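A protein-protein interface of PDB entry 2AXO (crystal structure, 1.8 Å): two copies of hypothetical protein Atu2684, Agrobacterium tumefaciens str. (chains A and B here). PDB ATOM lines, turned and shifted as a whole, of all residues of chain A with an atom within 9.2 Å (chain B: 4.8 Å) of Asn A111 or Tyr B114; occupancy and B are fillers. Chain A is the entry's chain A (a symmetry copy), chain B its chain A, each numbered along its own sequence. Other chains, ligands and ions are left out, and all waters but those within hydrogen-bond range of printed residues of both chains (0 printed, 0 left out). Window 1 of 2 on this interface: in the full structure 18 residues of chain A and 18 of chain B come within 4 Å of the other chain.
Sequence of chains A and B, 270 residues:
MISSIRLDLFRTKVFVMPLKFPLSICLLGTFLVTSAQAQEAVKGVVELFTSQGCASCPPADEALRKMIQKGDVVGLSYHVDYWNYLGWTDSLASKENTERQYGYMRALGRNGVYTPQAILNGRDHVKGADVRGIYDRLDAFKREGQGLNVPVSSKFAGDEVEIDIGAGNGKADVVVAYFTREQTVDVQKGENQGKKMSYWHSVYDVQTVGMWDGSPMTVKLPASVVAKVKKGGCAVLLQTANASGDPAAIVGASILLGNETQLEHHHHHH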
ATOM      1  N   GLN A 101     -22.501 -10.394 -19.168  1.00  0.00           N
ATOM      2  CA  GLN A 101     -21.231 -10.402 -18.459  1.00  0.00           C
ATOM      3  C   GLN A 101     -21.302  -9.404 -17.296  1.00  0.00           C
ATOM      4  O   GLN A 101     -20.665  -9.609 -16.264  1.00  0.00           O
ATOM      5  CB  GLN A 101     -20.067 -10.061 -19.394  1.00  0.00           C
ATOM      6  CG  GLN A 101     -18.700 -10.122 -18.726  1.00  0.00           C
ATOM      7  CD  GLN A 101     -17.567  -9.841 -19.699  1.00  0.00           C
ATOM      8  OE1 GLN A 101     -17.697  -9.004 -20.593  1.00  0.00           O
ATOM      9  NE2 GLN A 101     -16.442 -10.524 -19.515  1.00  0.00           N
ATOM     10  N   TYR A 102     -22.082  -8.333 -17.458  1.00  0.00           N
ATOM     11  CA  TYR A 102     -22.238  -7.347 -16.385  1.00  0.00           C
ATOM     12  C   TYR A 102     -23.007  -7.986 -15.235  1.00  0.00           C
ATOM     13  O   TYR A 102     -22.686  -7.784 -14.063  1.00  0.00           O
ATOM     14  CB  TYR A 102     -23.016  -6.113 -16.862  1.00  0.00           C
ATOM     15  CG  TYR A 102     -22.330  -5.300 -17.930  1.00  0.00           C
ATOM     16  CD1 TYR A 102     -20.942  -5.200 -17.977  1.00  0.00           C
ATOM     17  CD2 TYR A 102     -23.075  -4.582 -18.864  1.00  0.00           C
ATOM     18  CE1 TYR A 102     -20.310  -4.404 -18.927  1.00  0.00           C
ATOM     19  CE2 TYR A 102     -22.451  -3.779 -19.814  1.00  0.00           C
ATOM     20  CZ  TYR A 102     -21.067  -3.695 -19.834  1.00  0.00           C
ATOM     21  OH  TYR A 102     -20.444  -2.880 -20.751  1.00  0.00           O
ATOM     22  N   TYR A 104     -23.030 -11.003 -14.366  1.00  0.00           N
ATOM     23  CA  TYR A 104     -22.111 -11.870 -13.654  1.00  0.00           C
ATOM     24  C   TYR A 104     -21.140 -11.055 -12.813  1.00  0.00           C
ATOM     25  O   TYR A 104     -20.831 -11.429 -11.679  1.00  0.00           O
ATOM     26  CB  TYR A 104     -21.343 -12.765 -14.632  1.00  0.00           C
ATOM     27  CG  TYR A 104     -22.085 -14.035 -14.999  1.00  0.00           C
ATOM     28  CD1 TYR A 104     -22.597 -14.871 -14.009  1.00  0.00           C
ATOM     29  CD2 TYR A 104     -22.252 -14.413 -16.333  1.00  0.00           C
ATOM     30  CE1 TYR A 104     -23.259 -16.058 -14.336  1.00  0.00           C
ATOM     31  CE2 TYR A 104     -22.910 -15.596 -16.675  1.00  0.00           C
ATOM     32  CZ  TYR A 104     -23.409 -16.413 -15.675  1.00  0.00           C
ATOM     33  OH  TYR A 104     -24.045 -17.588 -16.005  1.00  0.00           O
ATOM     34  N   MET A 105     -20.657  -9.944 -13.360  1.00  0.00           N
ATOM     35  CA  MET A 105     -19.737  -9.087 -12.616  1.00  0.00           C
ATOM     36  C   MET A 105     -20.368  -8.729 -11.277  1.00  0.00           C
ATOM     37  O   MET A 105     -19.755  -8.890 -10.225  1.00  0.00           O
ATOM     38  CB  MET A 105     -19.446  -7.797 -13.388  1.00  0.00           C
ATOM     39  CG  MET A 105     -18.672  -6.753 -12.576  1.00  0.00           C
ATOM     40  SD  MET A 105     -18.655  -5.003 -13.416  1.00  0.00           S
ATOM     41  CE  MET A 105     -20.448  -4.485 -12.951  1.00  0.00           C
ATOM     42  N   ARG A 106     -21.601  -8.236 -11.326  1.00  0.00           N
ATOM     43  CA  ARG A 106     -22.303  -7.850 -10.114  1.00  0.00           C
ATOM     44  C   ARG A 106     -22.507  -9.023  -9.167  1.00  0.00           C
ATOM     45  O   ARG A 106     -22.188  -8.924  -7.985  1.00  0.00           O
ATOM     46  CB  ARG A 106     -23.652  -7.224 -10.460  1.00  0.00           C
ATOM     47  CG  ARG A 106     -23.545  -5.942 -11.268  1.00  0.00           C
ATOM     48  CD  ARG A 106     -24.881  -5.223 -11.319  1.00  0.00           C
ATOM     49  NE  ARG A 106     -25.872  -5.912 -12.138  1.00  0.00           N
ATOM     50  CZ  ARG A 106     -25.927  -5.836 -13.464  1.00  0.00           C
ATOM     51  NH1 ARG A 106     -25.044  -5.099 -14.128  1.00  0.00           N
ATOM     52  NH2 ARG A 106     -26.874  -6.484 -14.126  1.00  0.00           N
ATOM     53  N   ALA A 107     -23.031 -10.133  -9.679  1.00  0.00           N
ATOM     54  CA  ALA A 107     -23.264 -11.306  -8.842  1.00  0.00           C
ATOM     55  C   ALA A 107     -21.979 -11.802  -8.190  1.00  0.00           C
ATOM     56  O   ALA A 107     -21.985 -12.221  -7.035  1.00  0.00           O
ATOM     57  CB  ALA A 107     -23.893 -12.429  -9.666  1.00  0.00           C
ATOM     58  N   LEU A 108     -20.875 -11.755  -8.926  1.00  0.00           N
ATOM     59  CA  LEU A 108     -19.599 -12.223  -8.391  1.00  0.00           C
ATOM     60  C   LEU A 108     -18.926 -11.198  -7.476  1.00  0.00           C
ATOM     61  O   LEU A 108     -17.869 -11.464  -6.910  1.00  0.00           O
ATOM     62  CB  LEU A 108     -18.656 -12.599  -9.538  1.00  0.00           C
ATOM     63  CG  LEU A 108     -19.152 -13.736 -10.444  1.00  0.00           C
ATOM     64  CD1 LEU A 108     -18.149 -13.972 -11.564  1.00  0.00           C
ATOM     65  CD2 LEU A 108     -19.350 -15.010  -9.627  1.00  0.00           C
ATOM     66  N   GLY A 109     -19.548 -10.032  -7.333  1.00  0.00           N
ATOM     67  CA  GLY A 109     -18.996  -8.997  -6.477  1.00  0.00           C
ATOM     68  C   GLY A 109     -17.774  -8.285  -7.033  1.00  0.00           C
ATOM     69  O   GLY A 109     -17.031  -7.649  -6.281  1.00  0.00           O
ATOM     70  N   ARG A 110     -17.558  -8.378  -8.343  1.00  0.00           N
ATOM     71  CA  ARG A 110     -16.409  -7.723  -8.970  1.00  0.00           C
ATOM     72  C   ARG A 110     -16.735  -6.284  -9.372  1.00  0.00           C
ATOM     73  O   ARG A 110     -17.897  -5.885  -9.361  1.00  0.00           O
ATOM     74  CB  ARG A 110     -15.953  -8.524 -10.194  1.00  0.00           C
ATOM     75  CG  ARG A 110     -15.752 -10.005  -9.911  1.00  0.00           C
ATOM     76  CD  ARG A 110     -15.055 -10.719 -11.060  1.00  0.00           C
ATOM     77  NE  ARG A 110     -13.628 -10.404 -11.101  1.00  0.00           N
ATOM     78  CZ  ARG A 110     -13.036  -9.704 -12.062  1.00  0.00           C
ATOM     79  NH1 ARG A 110     -13.742  -9.236 -13.084  1.00  0.00           N
ATOM     80  NH2 ARG A 110     -11.733  -9.469 -11.999  1.00  0.00           N
ATOM     81  N   ASN A 111     -15.716  -5.500  -9.719  1.00  0.00           N
ATOM     82  CA  ASN A 111     -15.952  -4.110 -10.111  1.00  0.00           C
ATOM     83  C   ASN A 111     -15.549  -3.826 -11.551  1.00  0.00           C
ATOM     84  O   ASN A 111     -15.327  -2.672 -11.929  1.00  0.00           O
ATOM     85  CB  ASN A 111     -15.199  -3.154  -9.183  1.00  0.00           C
ATOM     86  CG  ASN A 111     -13.715  -3.103  -9.481  1.00  0.00           C
ATOM     87  OD1 ASN A 111     -13.037  -4.128  -9.486  1.00  0.00           O
ATOM     88  ND2 ASN A 111     -13.203  -1.904  -9.733  1.00  0.00           N
ATOM     89  N   GLY A 112     -15.447  -4.877 -12.355  1.00  0.00           N
ATOM     90  CA  GLY A 112     -15.076  -4.698 -13.746  1.00  0.00           C
ATOM     91  C   GLY A 112     -15.254  -5.958 -14.565  1.00  0.00           C
ATOM     92  O   GLY A 112     -15.628  -7.003 -14.036  1.00  0.00           O
ATOM     93  N   VAL A 113     -15.001  -5.847 -15.866  1.00  0.00           N
ATOM     94  CA  VAL A 113     -15.098  -6.982 -16.777  1.00  0.00           C
ATOM     95  C   VAL A 113     -13.851  -7.000 -17.652  1.00  0.00           C
ATOM     96  O   VAL A 113     -13.167  -5.984 -17.808  1.00  0.00           O
ATOM     97  CB  VAL A 113     -16.335  -6.887 -17.716  1.00  0.00           C
ATOM     98  CG1 VAL A 113     -17.621  -7.013 -16.915  1.00  0.00           C
ATOM     99  CG2 VAL A 113     -16.306  -5.570 -18.487  1.00  0.00           C
ATOM    100  N   TYR A 114     -13.560  -8.160 -18.224  1.00  0.00           N
ATOM    101  CA  TYR A 114     -12.407  -8.310 -19.093  1.00  0.00           C
ATOM    102  C   TYR A 114     -12.667  -9.467 -20.047  1.00  0.00           C
ATOM    103  O   TYR A 114     -13.615 -10.228 -19.866  1.00  0.00           O
ATOM    104  CB  TYR A 114     -11.144  -8.609 -18.272  1.00  0.00           C
ATOM    105  CG  TYR A 114     -11.167  -9.936 -17.535  1.00  0.00           C
ATOM    106  CD1 TYR A 114     -11.683 -10.038 -16.242  1.00  0.00           C
ATOM    107  CD2 TYR A 114     -10.691 -11.094 -18.144  1.00  0.00           C
ATOM    108  CE1 TYR A 114     -11.720 -11.269 -15.576  1.00  0.00           C
ATOM    109  CE2 TYR A 114     -10.727 -12.323 -17.491  1.00  0.00           C
ATOM    110  CZ  TYR A 114     -11.241 -12.406 -16.211  1.00  0.00           C
ATOM    111  OH  TYR A 114     -11.274 -13.628 -15.572  1.00  0.00           O
ATOM    112  N   GLN A 117     -12.939 -14.027 -20.600  1.00  0.00           N
ATOM    113  CA  GLN A 117     -13.363 -14.426 -19.268  1.00  0.00           C
ATOM    114  C   GLN A 117     -14.338 -15.587 -19.352  1.00  0.00           C
ATOM    115  O   GLN A 117     -15.324 -15.529 -20.085  1.00  0.00           O
ATOM    116  CB  GLN A 117     -14.051 -13.262 -18.553  1.00  0.00           C
ATOM    117  CG  GLN A 117     -14.620 -13.644 -17.195  1.00  0.00           C
ATOM    118  CD  GLN A 117     -15.362 -12.504 -16.528  1.00  0.00           C
ATOM    119  OE1 GLN A 117     -16.351 -11.999 -17.056  1.00  0.00           O
ATOM    120  NE2 GLN A 117     -14.893 -12.100 -15.354  1.00  0.00           N
ATOM    121  N   HIS A 125     -15.389 -17.117 -11.973  1.00  0.00           N
ATOM    122  CA  HIS A 125     -14.736 -16.741 -13.219  1.00  0.00           C
ATOM    123  C   HIS A 125     -13.273 -17.167 -13.235  1.00  0.00           C
ATOM    124  O   HIS A 125     -12.649 -17.336 -12.185  1.00  0.00           O
ATOM    125  CB  HIS A 125     -14.837 -15.228 -13.422  1.00  0.00           C
ATOM    126  CG  HIS A 125     -13.862 -14.445 -12.600  1.00  0.00           C
ATOM    127  ND1 HIS A 125     -12.707 -13.908 -13.129  1.00  0.00           N
ATOM    128  CD2 HIS A 125     -13.848 -14.145 -11.280  1.00  0.00           C
ATOM    129  CE1 HIS A 125     -12.022 -13.314 -12.169  1.00  0.00           C
ATOM    130  NE2 HIS A 125     -12.691 -13.444 -11.036  1.00  0.00           N
ATOM    131  N   SER B  56     -17.722   0.895  -4.536  1.00  0.00           N
ATOM    132  CA  SER B  56     -16.376   1.391  -4.276  1.00  0.00           C
ATOM    133  C   SER B  56     -16.100   2.709  -4.986  1.00  0.00           C
ATOM    134  O   SER B  56     -14.965   3.168  -5.026  1.00  0.00           O
ATOM    135  CB  SER B  56     -15.340   0.354  -4.716  1.00  0.00           C
ATOM    136  OG  SER B  56     -15.513   0.020  -6.083  1.00  0.00           O
ATOM    137  N   TYR B  82     -23.167  -0.144 -16.768  1.00  0.00           N
ATOM    138  CA  TYR B  82     -23.043  -1.535 -16.372  1.00  0.00           C
ATOM    139  C   TYR B  82     -23.197  -1.866 -14.890  1.00  0.00           C
ATOM    140  O   TYR B  82     -22.797  -2.938 -14.440  1.00  0.00           O
ATOM    141  CB  TYR B  82     -21.748  -2.132 -16.936  1.00  0.00           C
ATOM    142  CG  TYR B  82     -20.465  -1.395 -16.631  1.00  0.00           C
ATOM    143  CD1 TYR B  82     -19.888  -1.454 -15.365  1.00  0.00           C
ATOM    144  CD2 TYR B  82     -19.771  -0.734 -17.641  1.00  0.00           C
ATOM    145  CE1 TYR B  82     -18.640  -0.885 -15.117  1.00  0.00           C
ATOM    146  CE2 TYR B  82     -18.530  -0.160 -17.408  1.00  0.00           C
ATOM    147  CZ  TYR B  82     -17.966  -0.244 -16.149  1.00  0.00           C
ATOM    148  OH  TYR B  82     -16.712   0.273 -15.931  1.00  0.00           O
ATOM    149  N   TRP B  83     -23.796  -0.949 -14.138  1.00  0.00           N
ATOM    150  CA  TRP B  83     -24.039  -1.173 -12.719  1.00  0.00           C
ATOM    151  C   TRP B  83     -25.534  -1.128 -12.457  1.00  0.00           C
ATOM    152  O   TRP B  83     -25.983  -1.228 -11.315  1.00  0.00           O
ATOM    153  CB  TRP B  83     -23.331  -0.123 -11.860  1.00  0.00           C
ATOM    154  CG  TRP B  83     -21.879  -0.388 -11.698  1.00  0.00           C
ATOM    155  CD1 TRP B  83     -20.849   0.242 -12.341  1.00  0.00           C
ATOM    156  CD2 TRP B  83     -21.282  -1.372 -10.849  1.00  0.00           C
ATOM    157  NE1 TRP B  83     -19.649  -0.289 -11.942  1.00  0.00           N
ATOM    158  CE2 TRP B  83     -19.884  -1.281 -11.025  1.00  0.00           C
ATOM    159  CE3 TRP B  83     -21.793  -2.323  -9.956  1.00  0.00           C
ATOM    160  CZ2 TRP B  83     -18.985  -2.105 -10.335  1.00  0.00           C
ATOM    161  CZ3 TRP B  83     -20.899  -3.146  -9.270  1.00  0.00           C
ATOM    162  CH2 TRP B  83     -19.511  -3.028  -9.465  1.00  0.00           C
ATOM    163  N   GLN B 101     -15.594   4.842 -22.233  1.00  0.00           N
ATOM    164  CA  GLN B 101     -14.613   4.135 -21.423  1.00  0.00           C
ATOM    165  C   GLN B 101     -14.032   2.975 -22.242  1.00  0.00           C
ATOM    166  O   GLN B 101     -12.872   2.609 -22.061  1.00  0.00           O
ATOM    167  CB  GLN B 101     -15.232   3.621 -20.120  1.00  0.00           C
ATOM    168  CG  GLN B 101     -14.238   2.932 -19.194  1.00  0.00           C
ATOM    169  CD  GLN B 101     -14.874   2.493 -17.886  1.00  0.00           C
ATOM    170  OE1 GLN B 101     -16.028   2.064 -17.859  1.00  0.00           O
ATOM    171  NE2 GLN B 101     -14.115   2.578 -16.798  1.00  0.00           N
ATOM    172  N   ARG B 110      -5.620  -1.912 -22.990  1.00  0.00           N
ATOM    173  CA  ARG B 110      -6.102  -2.778 -21.913  1.00  0.00           C
ATOM    174  C   ARG B 110      -7.132  -3.787 -22.426  1.00  0.00           C
ATOM    175  O   ARG B 110      -7.616  -3.663 -23.548  1.00  0.00           O
ATOM    176  CB  ARG B 110      -6.707  -1.930 -20.790  1.00  0.00           C
ATOM    177  CG  ARG B 110      -5.800  -0.800 -20.325  1.00  0.00           C
ATOM    178  CD  ARG B 110      -6.307  -0.147 -19.047  1.00  0.00           C
ATOM    179  NE  ARG B 110      -6.064  -0.992 -17.880  1.00  0.00           N
ATOM    180  CZ  ARG B 110      -7.014  -1.579 -17.160  1.00  0.00           C
ATOM    181  NH1 ARG B 110      -8.293  -1.417 -17.477  1.00  0.00           N
ATOM    182  NH2 ARG B 110      -6.684  -2.332 -16.121  1.00  0.00           N
ATOM    183  N   GLY B 112      -9.926  -4.715 -20.459  1.00  0.00           N
ATOM    184  CA  GLY B 112     -11.099  -4.640 -19.611  1.00  0.00           C
ATOM    185  C   GLY B 112     -11.347  -3.245 -19.078  1.00  0.00           C
ATOM    186  O   GLY B 112     -10.568  -2.328 -19.334  1.00  0.00           O
ATOM    187  N   VAL B 113     -12.448  -3.086 -18.350  1.00  0.00           N
ATOM    188  CA  VAL B 113     -12.803  -1.808 -17.744  1.00  0.00           C
ATOM    189  C   VAL B 113     -13.199  -2.060 -16.294  1.00  0.00           C
ATOM    190  O   VAL B 113     -13.554  -3.180 -15.916  1.00  0.00           O
ATOM    191  CB  VAL B 113     -14.008  -1.127 -18.453  1.00  0.00           C
ATOM    192  CG1 VAL B 113     -13.629  -0.713 -19.865  1.00  0.00           C
ATOM    193  CG2 VAL B 113     -15.206  -2.072 -18.471  1.00  0.00           C
ATOM    194  N   TYR B 114     -13.138  -1.011 -15.485  1.00  0.00           N
ATOM    195  CA  TYR B 114     -13.502  -1.112 -14.083  1.00  0.00           C
ATOM    196  C   TYR B 114     -13.932   0.264 -13.595  1.00  0.00           C
ATOM    197  O   TYR B 114     -13.734   1.264 -14.283  1.00  0.00           O
ATOM    198  CB  TYR B 114     -12.308  -1.594 -13.246  1.00  0.00           C
ATOM    199  CG  TYR B 114     -11.134  -0.632 -13.206  1.00  0.00           C
ATOM    200  CD1 TYR B 114     -10.118  -0.689 -14.162  1.00  0.00           C
ATOM    201  CD2 TYR B 114     -11.054   0.350 -12.221  1.00  0.00           C
ATOM    202  CE1 TYR B 114      -9.049   0.214 -14.130  1.00  0.00           C
ATOM    203  CE2 TYR B 114      -9.996   1.254 -12.186  1.00  0.00           C
ATOM    204  CZ  TYR B 114      -8.999   1.184 -13.138  1.00  0.00           C
ATOM    205  OH  TYR B 114      -7.955   2.084 -13.096  1.00  0.00           O
ATOM    206  N   THR B 115     -14.544   0.309 -12.420  1.00  0.00           N
ATOM    207  CA  THR B 115     -14.943   1.578 -11.814  1.00  0.00           C
ATOM    208  C   THR B 115     -14.568   1.482 -10.344  1.00  0.00           C
ATOM    209  O   THR B 115     -14.664   0.416  -9.744  1.00  0.00           O
ATOM    210  CB  THR B 115     -16.473   1.859 -11.922  1.00  0.00           C
ATOM    211  OG1 THR B 115     -17.206   0.722 -11.455  1.00  0.00           O
ATOM    212  CG2 THR B 115     -16.870   2.187 -13.354  1.00  0.00           C
ATOM    213  N   PRO B 116     -14.107   2.592  -9.748  1.00  0.00           N
ATOM    214  CA  PRO B 116     -13.923   3.897 -10.386  1.00  0.00           C
ATOM    215  C   PRO B 116     -12.585   3.998 -11.114  1.00  0.00           C
ATOM    216  O   PRO B 116     -11.538   3.627 -10.572  1.00  0.00           O
ATOM    217  CB  PRO B 116     -14.018   4.864  -9.210  1.00  0.00           C
ATOM    218  CG  PRO B 116     -13.383   4.084  -8.106  1.00  0.00           C
ATOM    219  CD  PRO B 116     -13.945   2.694  -8.285  1.00  0.00           C
ATOM    220  N   GLN B 117     -12.628   4.496 -12.345  1.00  0.00           N
ATOM    221  CA  GLN B 117     -11.431   4.650 -13.155  1.00  0.00           C
ATOM    222  C   GLN B 117     -11.307   6.081 -13.646  1.00  0.00           C
ATOM    223  O   GLN B 117     -12.248   6.635 -14.213  1.00  0.00           O
ATOM    224  CB  GLN B 117     -11.482   3.721 -14.369  1.00  0.00           C
ATOM    225  CG  GLN B 117     -10.310   3.911 -15.321  1.00  0.00           C
ATOM    226  CD  GLN B 117     -10.408   3.038 -16.555  1.00  0.00           C
ATOM    227  OE1 GLN B 117     -11.354   3.147 -17.333  1.00  0.00           O
ATOM    228  NE2 GLN B 117      -9.421   2.172 -16.746  1.00  0.00           N
ATOM    229  N   HIS B 125      -4.582   5.809 -17.196  1.00  0.00           N
ATOM    230  CA  HIS B 125      -5.631   5.559 -16.217  1.00  0.00           C
ATOM    231  C   HIS B 125      -5.054   5.336 -14.824  1.00  0.00           C
ATOM    232  O   HIS B 125      -3.896   4.941 -14.672  1.00  0.00           O
ATOM    233  CB  HIS B 125      -6.453   4.338 -16.637  1.00  0.00           C
ATOM    234  CG  HIS B 125      -5.782   3.034 -16.348  1.00  0.00           C
ATOM    235  ND1 HIS B 125      -6.131   2.240 -15.275  1.00  0.00           N
ATOM    236  CD2 HIS B 125      -4.755   2.403 -16.965  1.00  0.00           C
ATOM    237  CE1 HIS B 125      -5.345   1.179 -15.242  1.00  0.00           C
ATOM    238  NE2 HIS B 125      -4.500   1.254 -16.256  1.00  0.00           N
ATOM    239  N   VAL B 126      -5.871   5.604 -13.811  1.00  0.00           N
ATOM    240  CA  VAL B 126      -5.476   5.442 -12.418  1.00  0.00           C
ATOM    241  C   VAL B 126      -6.727   5.245 -11.573  1.00  0.00           C
ATOM    242  O   VAL B 126      -7.827   5.608 -11.994  1.00  0.00           O
ATOM    243  CB  VAL B 126      -4.744   6.695 -11.884  1.00  0.00           C
ATOM    244  CG1 VAL B 126      -3.402   6.867 -12.578  1.00  0.00           C
ATOM    245  CG2 VAL B 126      -5.612   7.921 -12.092  1.00  0.00           C
ATOM    246  N   LYS B 127      -6.561   4.662 -10.391  1.00  0.00           N
ATOM    247  CA  LYS B 127      -7.693   4.462  -9.495  1.00  0.00           C
ATOM    248  C   LYS B 127      -8.347   5.819  -9.279  1.00  0.00           C
ATOM    249  O   LYS B 127      -7.662   6.812  -9.034  1.00  0.00           O
ATOM    250  CB  LYS B 127      -7.230   3.908  -8.147  1.00  0.00           C
ATOM    251  CG  LYS B 127      -6.951   2.417  -8.119  1.00  0.00           C
ATOM    252  CD  LYS B 127      -5.791   2.022  -9.009  1.00  0.00           C
ATOM    253  CE  LYS B 127      -5.319   0.608  -8.679  1.00  0.00           C
ATOM    254  NZ  LYS B 127      -6.429  -0.385  -8.730  1.00  0.00           N
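Tyr B82 touches Tyr A102. CE of Met A105 touches O of Tyr B82, at 3.2 Å. Met A105 touches Trp B83. Trp B83 touches Arg A110 (CH2 to O, 3.3 Å). Asn A111 touches Trp B83 (CA to CZ2, 3.6 Å). Tyr B114 touches Asn A111 (CA to O, 3.2 Å). CA of Gly A112 touches O of Val B113 (3.1 Å). CA of Gly A112 touches CA of Tyr B114, at 3.9 Å. Val A113 touches Gly B112 (O to CA, 3.1 Å). Tyr A114 touches Gly B112 (CA to CA, 3.9 Å).
Of chain B, only Trp B83, Tyr B114 and Thr B115 come within 4 Å of Asn A111. Tyr B114 touches just these residues of chain A: Asn A111 and Gly A112. Of chain A, only Gly A112 (3.1 Å) and Val A113 (3.0 Å) come within 4 Å of Val B113. Printed residues of chain B within 4 Å of Val A113: Gly B112 and Val B113. Printed residues of chain B within 4 Å of Tyr A114: Gly B112 (3.9 Å). Of the printed residues of chain A, Tyr B82 touches Tyr A102, Met A105 and Arg A106. Of the printed residues of chain B, Arg A110 touches Trp B83. Printed residues of chain A within 4 Å of Trp B83: Met A105 (3.8 Å), Arg A110 (3.3 Å) and Asn A111 (3.6 Å). Gln A101 touches none of the printed residues of chain B. The nearest residue of chain B that does not touch Asn A111 is Val B113 (4.4 Å). The nearest residue of chain A that does not touch Tyr B114 is Val A113 (5.2 Å). The nearest printed residue of chain B that does not touch Tyr A102 is Val B113 (5.6 Å).
O of Tyr A114 lies within hydrogen-bond range of NE2 of Gln A101. The indole nitrogen (NE1) of Trp B83 is in hydrogen-bond range of the side-chain hydroxyl (OG1) of Thr B115. The backbone carbonyl oxygen (O) of Gly A112 is in hydrogen-bond range of the guanidinium group (NH1) of Arg A110 (3.1 Å). The side-chain amide oxygen (OE1) of Gln B101 is in hydrogen-bond range of the side-chain hydroxyl (OH) of Tyr B82 (2.7 Å). The backbone carbonyl oxygen of Met A105 lies within hydrogen-bond range of the backbone NH of Arg A110 (2.9 Å). The guanidinium group (NE) of Arg A110 lies within hydrogen-bond range of a ring nitrogen (NE2) of His A125.
Printed residues of chain B that touch a printed residue of chain A: Tyr B82, Trp B83, Gly B112, Val B113, Tyr B114 and Thr B115. Hydrophobic or aromatic side chains of chain B that line the printed part of chain A: Tyr B82, Trp B83, Val B113 and Tyr B114. Hydrophobic or aromatic side chains of chain A within 4 Å of the printed part of chain B: Tyr A102, Met A105 and Val A113. Among the printed residues, no Asp or Glu carboxylate lies within 4 Å of a Lys or Arg side-chain nitrogen of the other chain.
Gly A112 touches Val B113, and with the chains exchanged Val A113 touches Gly B112. Gly A112 touches Tyr B114, and with the chains exchanged Tyr A114 touches Gly B112. Val B113 touches its own counterpart, Val A113. Positions printed for both chains: 101, 110, 112, 113, 114, 117 and 125. Of the 13 pairs that touch across the chains among the printed residues, 5 have their exchanged pair printed and touching as well.
The backbone NH (N) of Val B113 lies within hydrogen-bond range of the backbone carbonyl oxygen (O) of Val A113 (3.0 Å). NH1 of Arg A106 lies within hydrogen-bond range of O of Tyr B82 (3.1 Å). ND2 of Asn A111 lies within hydrogen-bond range of O of Thr B115 (2.7 Å).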
